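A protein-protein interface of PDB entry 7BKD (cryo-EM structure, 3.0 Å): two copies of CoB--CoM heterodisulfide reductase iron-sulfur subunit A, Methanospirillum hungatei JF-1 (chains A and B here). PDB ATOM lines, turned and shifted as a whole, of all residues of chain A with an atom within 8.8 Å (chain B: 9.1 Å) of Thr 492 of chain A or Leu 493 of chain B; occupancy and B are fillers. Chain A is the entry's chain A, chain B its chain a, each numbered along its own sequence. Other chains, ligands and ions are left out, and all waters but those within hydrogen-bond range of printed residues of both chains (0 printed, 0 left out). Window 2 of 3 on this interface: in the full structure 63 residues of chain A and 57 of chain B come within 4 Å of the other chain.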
ATOM      1  N   TYR A 444      21.065  21.917   1.542  1.00  0.00           N
ATOM      2  CA  TYR A 444      19.876  21.348   0.941  1.00  0.00           C
ATOM      3  C   TYR A 444      18.674  22.246   1.171  1.00  0.00           C
ATOM      4  O   TYR A 444      18.715  23.227   1.914  1.00  0.00           O
ATOM      5  CB  TYR A 444      19.590  19.947   1.500  1.00  0.00           C
ATOM      6  CG  TYR A 444      18.881  19.952   2.836  1.00  0.00           C
ATOM      7  CD1 TYR A 444      17.495  19.916   2.911  1.00  0.00           C
ATOM      8  CD2 TYR A 444      19.597  19.987   4.022  1.00  0.00           C
ATOM      9  CE1 TYR A 444      16.849  19.919   4.119  1.00  0.00           C
ATOM     10  CE2 TYR A 444      18.957  19.990   5.238  1.00  0.00           C
ATOM     11  CZ  TYR A 444      17.583  19.953   5.281  1.00  0.00           C
ATOM     12  OH  TYR A 444      16.933  19.956   6.492  1.00  0.00           O
ATOM     13  N   MET A 445      17.599  22.050   0.444  1.00  0.00           N
ATOM     14  CA  MET A 445      16.409  22.926   0.560  1.00  0.00           C
ATOM     15  C   MET A 445      15.246  22.022   0.205  1.00  0.00           C
ATOM     16  O   MET A 445      14.808  22.114  -0.962  1.00  0.00           O
ATOM     17  CB  MET A 445      16.509  24.022  -0.505  1.00  0.00           C
ATOM     18  CG  MET A 445      15.345  24.982  -0.586  1.00  0.00           C
ATOM     19  SD  MET A 445      15.581  26.054  -2.022  1.00  0.00           S
ATOM     20  CE  MET A 445      15.341  24.914  -3.380  1.00  0.00           C
ATOM     21  N   ASP A 446      14.884  21.085   1.074  1.00  0.00           N
ATOM     22  CA  ASP A 446      13.849  20.041   0.776  1.00  0.00           C
ATOM     23  C   ASP A 446      14.493  18.741   0.300  1.00  0.00           C
ATOM     24  O   ASP A 446      14.471  18.488  -0.906  1.00  0.00           O
ATOM     25  CB  ASP A 446      12.615  20.487  -0.025  1.00  0.00           C
ATOM     26  CG  ASP A 446      11.694  21.452   0.696  1.00  0.00           C
ATOM     27  OD1 ASP A 446      10.681  20.987   1.249  1.00  0.00           O
ATOM     28  OD2 ASP A 446      11.987  22.664   0.681  1.00  0.00           O
ATOM     29  N   PHE A 468      23.771  18.204   7.414  1.00  0.00           N
ATOM     30  CA  PHE A 468      22.711  18.755   6.577  1.00  0.00           C
ATOM     31  C   PHE A 468      22.391  20.165   7.047  1.00  0.00           C
ATOM     32  O   PHE A 468      21.812  20.349   8.121  1.00  0.00           O
ATOM     33  CB  PHE A 468      21.459  17.879   6.603  1.00  0.00           C
ATOM     34  CG  PHE A 468      21.651  16.520   5.998  1.00  0.00           C
ATOM     35  CD1 PHE A 468      22.437  15.568   6.624  1.00  0.00           C
ATOM     36  CD2 PHE A 468      21.077  16.210   4.779  1.00  0.00           C
ATOM     37  CE1 PHE A 468      22.618  14.324   6.067  1.00  0.00           C
ATOM     38  CE2 PHE A 468      21.262  14.970   4.211  1.00  0.00           C
ATOM     39  CZ  PHE A 468      22.034  14.024   4.858  1.00  0.00           C
ATOM     40  N   ILE A 469      22.757  21.155   6.240  1.00  0.00           N
ATOM     41  CA  ILE A 469      22.409  22.548   6.489  1.00  0.00           C
ATOM     42  C   ILE A 469      21.245  22.903   5.580  1.00  0.00           C
ATOM     43  O   ILE A 469      21.377  22.879   4.351  1.00  0.00           O
ATOM     44  CB  ILE A 469      23.606  23.485   6.251  1.00  0.00           C
ATOM     45  CG1 ILE A 469      24.709  23.224   7.276  1.00  0.00           C
ATOM     46  CG2 ILE A 469      23.169  24.936   6.309  1.00  0.00           C
ATOM     47  CD1 ILE A 469      25.746  22.232   6.826  1.00  0.00           C
ATOM     48  N   ARG A 470      20.103  23.228   6.178  1.00  0.00           N
ATOM     49  CA  ARG A 470      18.897  23.560   5.422  1.00  0.00           C
ATOM     50  C   ARG A 470      18.984  25.014   4.981  1.00  0.00           C
ATOM     51  O   ARG A 470      18.479  25.923   5.639  1.00  0.00           O
ATOM     52  CB  ARG A 470      17.651  23.299   6.254  1.00  0.00           C
ATOM     53  CG  ARG A 470      16.392  23.111   5.436  1.00  0.00           C
ATOM     54  CD  ARG A 470      15.527  24.325   5.515  1.00  0.00           C
ATOM     55  NE  ARG A 470      14.328  24.235   4.696  1.00  0.00           N
ATOM     56  CZ  ARG A 470      13.678  25.298   4.236  1.00  0.00           C
ATOM     57  NH1 ARG A 470      14.130  26.511   4.513  1.00  0.00           N
ATOM     58  NH2 ARG A 470      12.592  25.153   3.496  1.00  0.00           N
ATOM     59  N   GLY A 471      19.642  25.231   3.847  1.00  0.00           N
ATOM     60  CA  GLY A 471      19.728  26.545   3.248  1.00  0.00           C
ATOM     61  C   GLY A 471      20.294  26.513   1.845  1.00  0.00           C
ATOM     62  O   GLY A 471      21.329  25.888   1.597  1.00  0.00           O
ATOM     63  N   ARG A 472      19.615  27.177   0.915  1.00  0.00           N
ATOM     64  CA  ARG A 472      20.138  27.322  -0.433  1.00  0.00           C
ATOM     65  C   ARG A 472      21.357  28.233  -0.420  1.00  0.00           C
ATOM     66  O   ARG A 472      21.352  29.290   0.214  1.00  0.00           O
ATOM     67  CB  ARG A 472      19.062  27.882  -1.358  1.00  0.00           C
ATOM     68  CG  ARG A 472      19.331  27.665  -2.831  1.00  0.00           C
ATOM     69  CD  ARG A 472      18.227  28.268  -3.669  1.00  0.00           C
ATOM     70  NE  ARG A 472      18.611  28.401  -5.069  1.00  0.00           N
ATOM     71  CZ  ARG A 472      19.191  29.478  -5.585  1.00  0.00           C
ATOM     72  NH1 ARG A 472      19.463  30.518  -4.814  1.00  0.00           N
ATOM     73  NH2 ARG A 472      19.502  29.512  -6.870  1.00  0.00           N
ATOM     74  N   THR A 489      25.677  31.012   2.979  1.00  0.00           N
ATOM     75  CA  THR A 489      24.233  30.817   2.947  1.00  0.00           C
ATOM     76  C   THR A 489      23.700  31.068   4.352  1.00  0.00           C
ATOM     77  O   THR A 489      24.387  31.645   5.198  1.00  0.00           O
ATOM     78  CB  THR A 489      23.864  29.424   2.420  1.00  0.00           C
ATOM     79  OG1 THR A 489      22.449  29.229   2.523  1.00  0.00           O
ATOM     80  CG2 THR A 489      24.585  28.332   3.185  1.00  0.00           C
ATOM     81  N   GLU A 490      22.461  30.666   4.595  1.00  0.00           N
ATOM     82  CA  GLU A 490      21.886  30.701   5.928  1.00  0.00           C
ATOM     83  C   GLU A 490      21.435  29.305   6.326  1.00  0.00           C
ATOM     84  O   GLU A 490      20.865  28.573   5.514  1.00  0.00           O
ATOM     85  CB  GLU A 490      20.692  31.652   6.013  1.00  0.00           C
ATOM     86  CG  GLU A 490      20.182  31.839   7.432  1.00  0.00           C
ATOM     87  CD  GLU A 490      18.740  32.294   7.487  1.00  0.00           C
ATOM     88  OE1 GLU A 490      18.274  32.674   8.582  1.00  0.00           O
ATOM     89  OE2 GLU A 490      18.069  32.269   6.435  1.00  0.00           O
ATOM     90  N   ASP A 491      21.698  28.939   7.577  1.00  0.00           N
ATOM     91  CA  ASP A 491      21.051  27.790   8.198  1.00  0.00           C
ATOM     92  C   ASP A 491      19.713  28.295   8.722  1.00  0.00           C
ATOM     93  O   ASP A 491      19.638  28.897   9.799  1.00  0.00           O
ATOM     94  CB  ASP A 491      21.922  27.205   9.303  1.00  0.00           C
ATOM     95  CG  ASP A 491      21.706  25.715   9.492  1.00  0.00           C
ATOM     96  OD1 ASP A 491      22.493  25.092  10.233  1.00  0.00           O
ATOM     97  OD2 ASP A 491      20.743  25.167   8.913  1.00  0.00           O
ATOM     98  N   THR A 492      18.660  28.089   7.924  1.00  0.00           N
ATOM     99  CA  THR A 492      17.335  28.584   8.278  1.00  0.00           C
ATOM    100  C   THR A 492      16.801  27.885   9.520  1.00  0.00           C
ATOM    101  O   THR A 492      16.176  28.518  10.377  1.00  0.00           O
ATOM    102  CB  THR A 492      16.376  28.410   7.103  1.00  0.00           C
ATOM    103  OG1 THR A 492      16.085  27.020   6.930  1.00  0.00           O
ATOM    104  CG2 THR A 492      16.990  28.957   5.823  1.00  0.00           C
ATOM    105  N   LEU A 493      17.005  26.576   9.617  1.00  0.00           N
ATOM    106  CA  LEU A 493      16.981  25.928  10.919  1.00  0.00           C
ATOM    107  C   LEU A 493      18.258  26.316  11.644  1.00  0.00           C
ATOM    108  O   LEU A 493      19.337  26.301  11.050  1.00  0.00           O
ATOM    109  CB  LEU A 493      16.876  24.412  10.768  1.00  0.00           C
ATOM    110  CG  LEU A 493      15.870  23.932   9.725  1.00  0.00           C
ATOM    111  CD1 LEU A 493      16.040  22.451   9.459  1.00  0.00           C
ATOM    112  CD2 LEU A 493      14.457  24.247  10.163  1.00  0.00           C
ATOM    113  N   LEU A 494      18.136  26.667  12.920  1.00  0.00           N
ATOM    114  CA  LEU A 494      19.098  27.398  13.740  1.00  0.00           C
ATOM    115  C   LEU A 494      19.084  28.891  13.423  1.00  0.00           C
ATOM    116  O   LEU A 494      19.583  29.674  14.227  1.00  0.00           O
ATOM    117  CB  LEU A 494      20.545  26.883  13.587  1.00  0.00           C
ATOM    118  CG  LEU A 494      21.700  27.457  14.408  1.00  0.00           C
ATOM    119  CD1 LEU A 494      21.575  27.077  15.876  1.00  0.00           C
ATOM    120  CD2 LEU A 494      23.041  27.038  13.827  1.00  0.00           C
ATOM    121  N   GLY A 495      18.456  29.320  12.330  1.00  0.00           N
ATOM    122  CA  GLY A 495      18.282  30.724  12.009  1.00  0.00           C
ATOM    123  C   GLY A 495      19.518  31.604  12.045  1.00  0.00           C
ATOM    124  O   GLY A 495      19.467  32.699  12.610  1.00  0.00           O
ATOM    125  N   ARG A 496      20.632  31.162  11.470  1.00  0.00           N
ATOM    126  CA  ARG A 496      21.836  31.984  11.510  1.00  0.00           C
ATOM    127  C   ARG A 496      22.546  31.956  10.166  1.00  0.00           C
ATOM    128  O   ARG A 496      22.538  30.931   9.477  1.00  0.00           O
ATOM    129  CB  ARG A 496      22.816  31.529  12.609  1.00  0.00           C
ATOM    130  CG  ARG A 496      22.181  31.302  13.979  1.00  0.00           C
ATOM    131  CD  ARG A 496      23.197  30.967  15.068  1.00  0.00           C
ATOM    132  NE  ARG A 496      24.509  31.549  14.813  1.00  0.00           N
ATOM    133  CZ  ARG A 496      25.656  31.005  15.204  1.00  0.00           C
ATOM    134  NH1 ARG A 496      25.660  29.863  15.876  1.00  0.00           N
ATOM    135  NH2 ARG A 496      26.802  31.605  14.925  1.00  0.00           N
ATOM    136  N   PRO A 497      23.183  33.059   9.778  1.00  0.00           N
ATOM    137  CA  PRO A 497      24.050  33.028   8.596  1.00  0.00           C
ATOM    138  C   PRO A 497      25.219  32.083   8.818  1.00  0.00           C
ATOM    139  O   PRO A 497      25.641  31.842   9.949  1.00  0.00           O
ATOM    140  CB  PRO A 497      24.522  34.481   8.457  1.00  0.00           C
ATOM    141  CG  PRO A 497      23.551  35.281   9.245  1.00  0.00           C
ATOM    142  CD  PRO A 497      23.083  34.408  10.356  1.00  0.00           C
ATOM    143  N   VAL A 498      25.741  31.540   7.725  1.00  0.00           N
ATOM    144  CA  VAL A 498      26.774  30.518   7.810  1.00  0.00           C
ATOM    145  C   VAL A 498      27.740  30.688   6.644  1.00  0.00           C
ATOM    146  O   VAL A 498      27.333  30.962   5.506  1.00  0.00           O
ATOM    147  CB  VAL A 498      26.146  29.104   7.850  1.00  0.00           C
ATOM    148  CG1 VAL A 498      25.292  28.856   6.630  1.00  0.00           C
ATOM    149  CG2 VAL A 498      27.206  28.045   7.979  1.00  0.00           C
ATOM    150  N   TYR B 444       3.802  20.689   7.166  1.00  0.00           N
ATOM    151  CA  TYR B 444       4.594  19.847   6.296  1.00  0.00           C
ATOM    152  C   TYR B 444       6.007  19.695   6.829  1.00  0.00           C
ATOM    153  O   TYR B 444       6.422  20.336   7.796  1.00  0.00           O
ATOM    154  CB  TYR B 444       4.634  20.413   4.869  1.00  0.00           C
ATOM    155  CG  TYR B 444       5.624  21.540   4.680  1.00  0.00           C
ATOM    156  CD1 TYR B 444       5.251  22.858   4.896  1.00  0.00           C
ATOM    157  CD2 TYR B 444       6.931  21.287   4.286  1.00  0.00           C
ATOM    158  CE1 TYR B 444       6.149  23.888   4.726  1.00  0.00           C
ATOM    159  CE2 TYR B 444       7.830  22.307   4.115  1.00  0.00           C
ATOM    160  CZ  TYR B 444       7.436  23.607   4.334  1.00  0.00           C
ATOM    161  OH  TYR B 444       8.342  24.627   4.162  1.00  0.00           O
ATOM    162  N   ASP B 446       9.513  18.764   4.429  1.00  0.00           N
ATOM    163  CA  ASP B 446      10.045  18.353   3.127  1.00  0.00           C
ATOM    164  C   ASP B 446       8.917  18.070   2.127  1.00  0.00           C
ATOM    165  O   ASP B 446       8.604  16.922   1.814  1.00  0.00           O
ATOM    166  CB  ASP B 446      10.967  17.132   3.255  1.00  0.00           C
ATOM    167  CG  ASP B 446      12.168  17.397   4.128  1.00  0.00           C
ATOM    168  OD1 ASP B 446      13.154  17.974   3.626  1.00  0.00           O
ATOM    169  OD2 ASP B 446      12.128  17.023   5.318  1.00  0.00           O
ATOM    170  N   TYR B 458       2.954  22.749  -7.086  1.00  0.00           N
ATOM    171  CA  TYR B 458       3.289  23.353  -5.800  1.00  0.00           C
ATOM    172  C   TYR B 458       3.289  24.877  -5.891  1.00  0.00           C
ATOM    173  O   TYR B 458       2.763  25.565  -5.004  1.00  0.00           O
ATOM    174  CB  TYR B 458       4.651  22.813  -5.362  1.00  0.00           C
ATOM    175  CG  TYR B 458       5.235  23.367  -4.090  1.00  0.00           C
ATOM    176  CD1 TYR B 458       4.435  23.682  -3.004  1.00  0.00           C
ATOM    177  CD2 TYR B 458       6.606  23.541  -3.968  1.00  0.00           C
ATOM    178  CE1 TYR B 458       4.984  24.176  -1.842  1.00  0.00           C
ATOM    179  CE2 TYR B 458       7.161  24.031  -2.812  1.00  0.00           C
ATOM    180  CZ  TYR B 458       6.347  24.349  -1.751  1.00  0.00           C
ATOM    181  OH  TYR B 458       6.904  24.841  -0.597  1.00  0.00           O
ATOM    182  N   PHE B 468       1.883  27.369   4.301  1.00  0.00           N
ATOM    183  CA  PHE B 468       2.792  26.252   4.522  1.00  0.00           C
ATOM    184  C   PHE B 468       3.568  26.498   5.807  1.00  0.00           C
ATOM    185  O   PHE B 468       4.453  27.358   5.848  1.00  0.00           O
ATOM    186  CB  PHE B 468       3.742  26.063   3.341  1.00  0.00           C
ATOM    187  CG  PHE B 468       3.074  25.549   2.102  1.00  0.00           C
ATOM    188  CD1 PHE B 468       2.228  26.362   1.368  1.00  0.00           C
ATOM    189  CD2 PHE B 468       3.262  24.242   1.691  1.00  0.00           C
ATOM    190  CE1 PHE B 468       1.610  25.895   0.232  1.00  0.00           C
ATOM    191  CE2 PHE B 468       2.638  23.765   0.559  1.00  0.00           C
ATOM    192  CZ  PHE B 468       1.810  24.595  -0.172  1.00  0.00           C
ATOM    193  N   ILE B 469       3.245  25.740   6.848  1.00  0.00           N
ATOM    194  CA  ILE B 469       3.963  25.786   8.114  1.00  0.00           C
ATOM    195  C   ILE B 469       4.902  24.590   8.143  1.00  0.00           C
ATOM    196  O   ILE B 469       4.455  23.439   8.173  1.00  0.00           O
ATOM    197  CB  ILE B 469       3.009  25.782   9.316  1.00  0.00           C
ATOM    198  CG1 ILE B 469       2.152  27.048   9.338  1.00  0.00           C
ATOM    199  CG2 ILE B 469       3.782  25.644  10.614  1.00  0.00           C
ATOM    200  CD1 ILE B 469       0.840  26.924   8.607  1.00  0.00           C
ATOM    201  N   ARG B 470       6.203  24.855   8.133  1.00  0.00           N
ATOM    202  CA  ARG B 470       7.207  23.794   8.142  1.00  0.00           C
ATOM    203  C   ARG B 470       7.385  23.312   9.574  1.00  0.00           C
ATOM    204  O   ARG B 470       8.260  23.771  10.309  1.00  0.00           O
ATOM    205  CB  ARG B 470       8.519  24.285   7.548  1.00  0.00           C
ATOM    206  CG  ARG B 470       9.424  23.178   7.053  1.00  0.00           C
ATOM    207  CD  ARG B 470      10.542  22.941   8.016  1.00  0.00           C
ATOM    208  NE  ARG B 470      11.466  21.907   7.573  1.00  0.00           N
ATOM    209  CZ  ARG B 470      12.262  21.241   8.399  1.00  0.00           C
ATOM    210  NH1 ARG B 470      12.228  21.503   9.695  1.00  0.00           N
ATOM    211  NH2 ARG B 470      13.081  20.309   7.938  1.00  0.00           N
ATOM    212  N   GLY B 471       6.534  22.374   9.973  1.00  0.00           N
ATOM    213  CA  GLY B 471       6.639  21.745  11.271  1.00  0.00           C
ATOM    214  C   GLY B 471       5.746  20.532  11.404  1.00  0.00           C
ATOM    215  O   GLY B 471       4.555  20.588  11.085  1.00  0.00           O
ATOM    216  N   ARG B 472       6.316  19.424  11.869  1.00  0.00           N
ATOM    217  CA  ARG B 472       5.529  18.230  12.130  1.00  0.00           C
ATOM    218  C   ARG B 472       4.599  18.465  13.311  1.00  0.00           C
ATOM    219  O   ARG B 472       5.010  18.994  14.347  1.00  0.00           O
ATOM    220  CB  ARG B 472       6.447  17.043  12.402  1.00  0.00           C
ATOM    221  CG  ARG B 472       5.751  15.700  12.381  1.00  0.00           C
ATOM    222  CD  ARG B 472       6.751  14.572  12.519  1.00  0.00           C
ATOM    223  NE  ARG B 472       6.100  13.294  12.777  1.00  0.00           N
ATOM    224  CZ  ARG B 472       5.659  12.908  13.968  1.00  0.00           C
ATOM    225  NH1 ARG B 472       5.801  13.701  15.017  1.00  0.00           N
ATOM    226  NH2 ARG B 472       5.078  11.727  14.110  1.00  0.00           N
ATOM    227  N   GLU B 490       5.484  23.364  16.044  1.00  0.00           N
ATOM    228  CA  GLU B 490       6.356  24.506  15.847  1.00  0.00           C
ATOM    229  C   GLU B 490       6.336  24.874  14.372  1.00  0.00           C
ATOM    230  O   GLU B 490       6.245  24.001  13.507  1.00  0.00           O
ATOM    231  CB  GLU B 490       7.807  24.214  16.239  1.00  0.00           C
ATOM    232  CG  GLU B 490       8.704  25.444  16.132  1.00  0.00           C
ATOM    233  CD  GLU B 490      10.151  25.172  16.472  1.00  0.00           C
ATOM    234  OE1 GLU B 490      10.492  24.004  16.735  1.00  0.00           O
ATOM    235  OE2 GLU B 490      10.950  26.132  16.491  1.00  0.00           O
ATOM    236  N   ASP B 491       6.425  26.162  14.082  1.00  0.00           N
ATOM    237  CA  ASP B 491       6.795  26.601  12.747  1.00  0.00           C
ATOM    238  C   ASP B 491       8.300  26.806  12.885  1.00  0.00           C
ATOM    239  O   ASP B 491       8.752  27.795  13.472  1.00  0.00           O
ATOM    240  CB  ASP B 491       6.047  27.867  12.338  1.00  0.00           C
ATOM    241  CG  ASP B 491       6.334  28.292  10.905  1.00  0.00           C
ATOM    242  OD1 ASP B 491       7.258  27.740  10.269  1.00  0.00           O
ATOM    243  OD2 ASP B 491       5.625  29.195  10.415  1.00  0.00           O
ATOM    244  N   THR B 492       9.071  25.815  12.421  1.00  0.00           N
ATOM    245  CA  THR B 492      10.517  25.820  12.628  1.00  0.00           C
ATOM    246  C   THR B 492      11.171  26.980  11.899  1.00  0.00           C
ATOM    247  O   THR B 492      12.093  27.613  12.423  1.00  0.00           O
ATOM    248  CB  THR B 492      11.124  24.496  12.166  1.00  0.00           C
ATOM    249  OG1 THR B 492      10.991  24.386  10.746  1.00  0.00           O
ATOM    250  CG2 THR B 492      10.420  23.322  12.827  1.00  0.00           C
ATOM    251  N   LEU B 493      10.735  27.242  10.677  1.00  0.00           N
ATOM    252  CA  LEU B 493      10.982  28.532  10.059  1.00  0.00           C
ATOM    253  C   LEU B 493      10.162  29.561  10.821  1.00  0.00           C
ATOM    254  O   LEU B 493       9.044  29.272  11.240  1.00  0.00           O
ATOM    255  CB  LEU B 493      10.579  28.469   8.592  1.00  0.00           C
ATOM    256  CG  LEU B 493      11.483  27.486   7.845  1.00  0.00           C
ATOM    257  CD1 LEU B 493      11.028  27.284   6.422  1.00  0.00           C
ATOM    258  CD2 LEU B 493      12.926  27.931   7.897  1.00  0.00           C
ATOM    259  N   LEU B 494      10.739  30.740  11.055  1.00  0.00           N
ATOM    260  CA  LEU B 494      10.196  31.722  12.001  1.00  0.00           C
ATOM    261  C   LEU B 494      10.436  31.276  13.440  1.00  0.00           C
ATOM    262  O   LEU B 494      10.286  32.072  14.370  1.00  0.00           O
ATOM    263  CB  LEU B 494       8.694  31.955  11.779  1.00  0.00           C
ATOM    264  CG  LEU B 494       7.912  32.999  12.576  1.00  0.00           C
ATOM    265  CD1 LEU B 494       8.323  34.414  12.200  1.00  0.00           C
ATOM    266  CD2 LEU B 494       6.415  32.787  12.422  1.00  0.00           C
ATOM    267  N   GLY B 495      10.858  30.025  13.621  1.00  0.00           N
ATOM    268  CA  GLY B 495      11.179  29.447  14.913  1.00  0.00           C
ATOM    269  C   GLY B 495      10.256  29.774  16.070  1.00  0.00           C
ATOM    270  O   GLY B 495      10.712  30.311  17.083  1.00  0.00           O
ATOM    271  N   ARG B 496       8.970  29.464  15.955  1.00  0.00           N
ATOM    272  CA  ARG B 496       8.070  29.769  17.060  1.00  0.00           C
ATOM    273  C   ARG B 496       7.051  28.655  17.239  1.00  0.00           C
ATOM    274  O   ARG B 496       6.623  28.038  16.259  1.00  0.00           O
ATOM    275  CB  ARG B 496       7.329  31.099  16.846  1.00  0.00           C
ATOM    276  CG  ARG B 496       8.051  32.315  17.396  1.00  0.00           C
ATOM    277  CD  ARG B 496       7.477  33.603  16.826  1.00  0.00           C
ATOM    278  NE  ARG B 496       6.127  33.846  17.316  1.00  0.00           N
ATOM    279  CZ  ARG B 496       5.299  34.754  16.813  1.00  0.00           C
ATOM    280  NH1 ARG B 496       5.680  35.512  15.796  1.00  0.00           N
ATOM    281  NH2 ARG B 496       4.088  34.900  17.326  1.00  0.00           N
ATOM    282  N   PRO B 497       6.632  28.391  18.475  1.00  0.00           N
ATOM    283  CA  PRO B 497       5.499  27.485  18.684  1.00  0.00           C
ATOM    284  C   PRO B 497       4.237  28.051  18.054  1.00  0.00           C
ATOM    285  O   PRO B 497       4.066  29.264  17.935  1.00  0.00           O
ATOM    286  CB  PRO B 497       5.382  27.402  20.211  1.00  0.00           C
ATOM    287  CG  PRO B 497       6.129  28.585  20.722  1.00  0.00           C
ATOM    288  CD  PRO B 497       7.230  28.824  19.747  1.00  0.00           C
ATOM    289  N   VAL B 498       3.354  27.151  17.627  1.00  0.00           N
ATOM    290  CA  VAL B 498       2.174  27.495  16.846  1.00  0.00           C
ATOM    291  C   VAL B 498       0.994  26.677  17.353  1.00  0.00           C
ATOM    292  O   VAL B 498       1.113  25.462  17.555  1.00  0.00           O
ATOM    293  CB  VAL B 498       2.393  27.238  15.339  1.00  0.00           C
ATOM    294  CG1 VAL B 498       1.161  27.597  14.556  1.00  0.00           C
ATOM    295  CG2 VAL B 498       3.576  28.023  14.825  1.00  0.00           C
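Printed residues of chain B that touch a printed residue of chain A: Asp 446, Arg 470, Thr 492 and Leu 493. Along chain A the printed residues that touch a printed residue of chain B span positions 446 to 493. Among the printed residues, no Asp or Glu carboxylate lies within 4 Å of a Lys or Arg side-chain nitrogen of the other chain.
Thr 492 of chain A touches just one residue of chain B: Leu 493. Of chain A, only Arg 470 (3.7 Å) and Thr 492 (3.4 Å) come within 4 Å of Leu 493 of chain B. Of the printed residues of chain A, Thr 492 of chain B touches Leu 493 (3.5 Å). Printed residues of chain B within 4 Å of Asp 446 of chain A: Asp 446. Of the printed residues of chain B, Leu 493 of chain A touches Arg 470 and Thr 492. Printed residues of chain B within 4 Å of Arg 470 of chain A: Leu 493 (3.7 Å). Printed residues of chain A within 4 Å of Asp 446 of chain B: Asp 446 (3.3 Å). Of the printed residues of chain A, Arg 470 of chain B touches Leu 493 (3.6 Å). Tyr 444 of chain A touches none of the printed residues of chain B. Val 498 of chain A touches none of the printed residues of chain B. The nearest residue of chain A that does not touch Leu 493 of chain B is Leu 493 of chain A (4.6 Å). The nearest printed residue of chain B that does not touch Arg 470 of chain A is Tyr 444 of chain B (4.3 Å).
OD2 of Asp 446 of chain A is in salt-bridge range of NH2 of Arg 470 of chain A (3.8 Å). OD2 of Asp 491 of chain A is in hydrogen-bond range of N of Arg 470 of chain A (3.4 Å). OG1 of Thr 492 of chain A sits at hydrogen-bond distance from O of Arg 470 of chain A. O of Arg 470 of chain B lies within hydrogen-bond range of OG1 of Thr 492 of chain B (2.8 Å). OD1 of Asp 491 of chain B lies close to O of Leu 493 of chain B.
Among the printed residues, merely in contact across the chains: Asp 446 of chain A with Asp 446 of chain B, Arg 470 of chain A with Leu 493 of chain B, Thr 492 of chain A with Leu 493 of chain B, Leu 493 of chain A with Arg 470 of chain B and Leu 493 of chain A with Thr 492 of chain B.
Asp 446 of chain A touches its own counterpart, Asp 446 of chain B. Arg 470 of chain A touches Leu 493 of chain B, and with the chains exchanged Leu 493 of chain A touches Arg 470 of chain B. Thr 492 of chain A touches Leu 493 of chain B, and with the chains exchanged Leu 493 of chain A touches Thr 492 of chain B.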
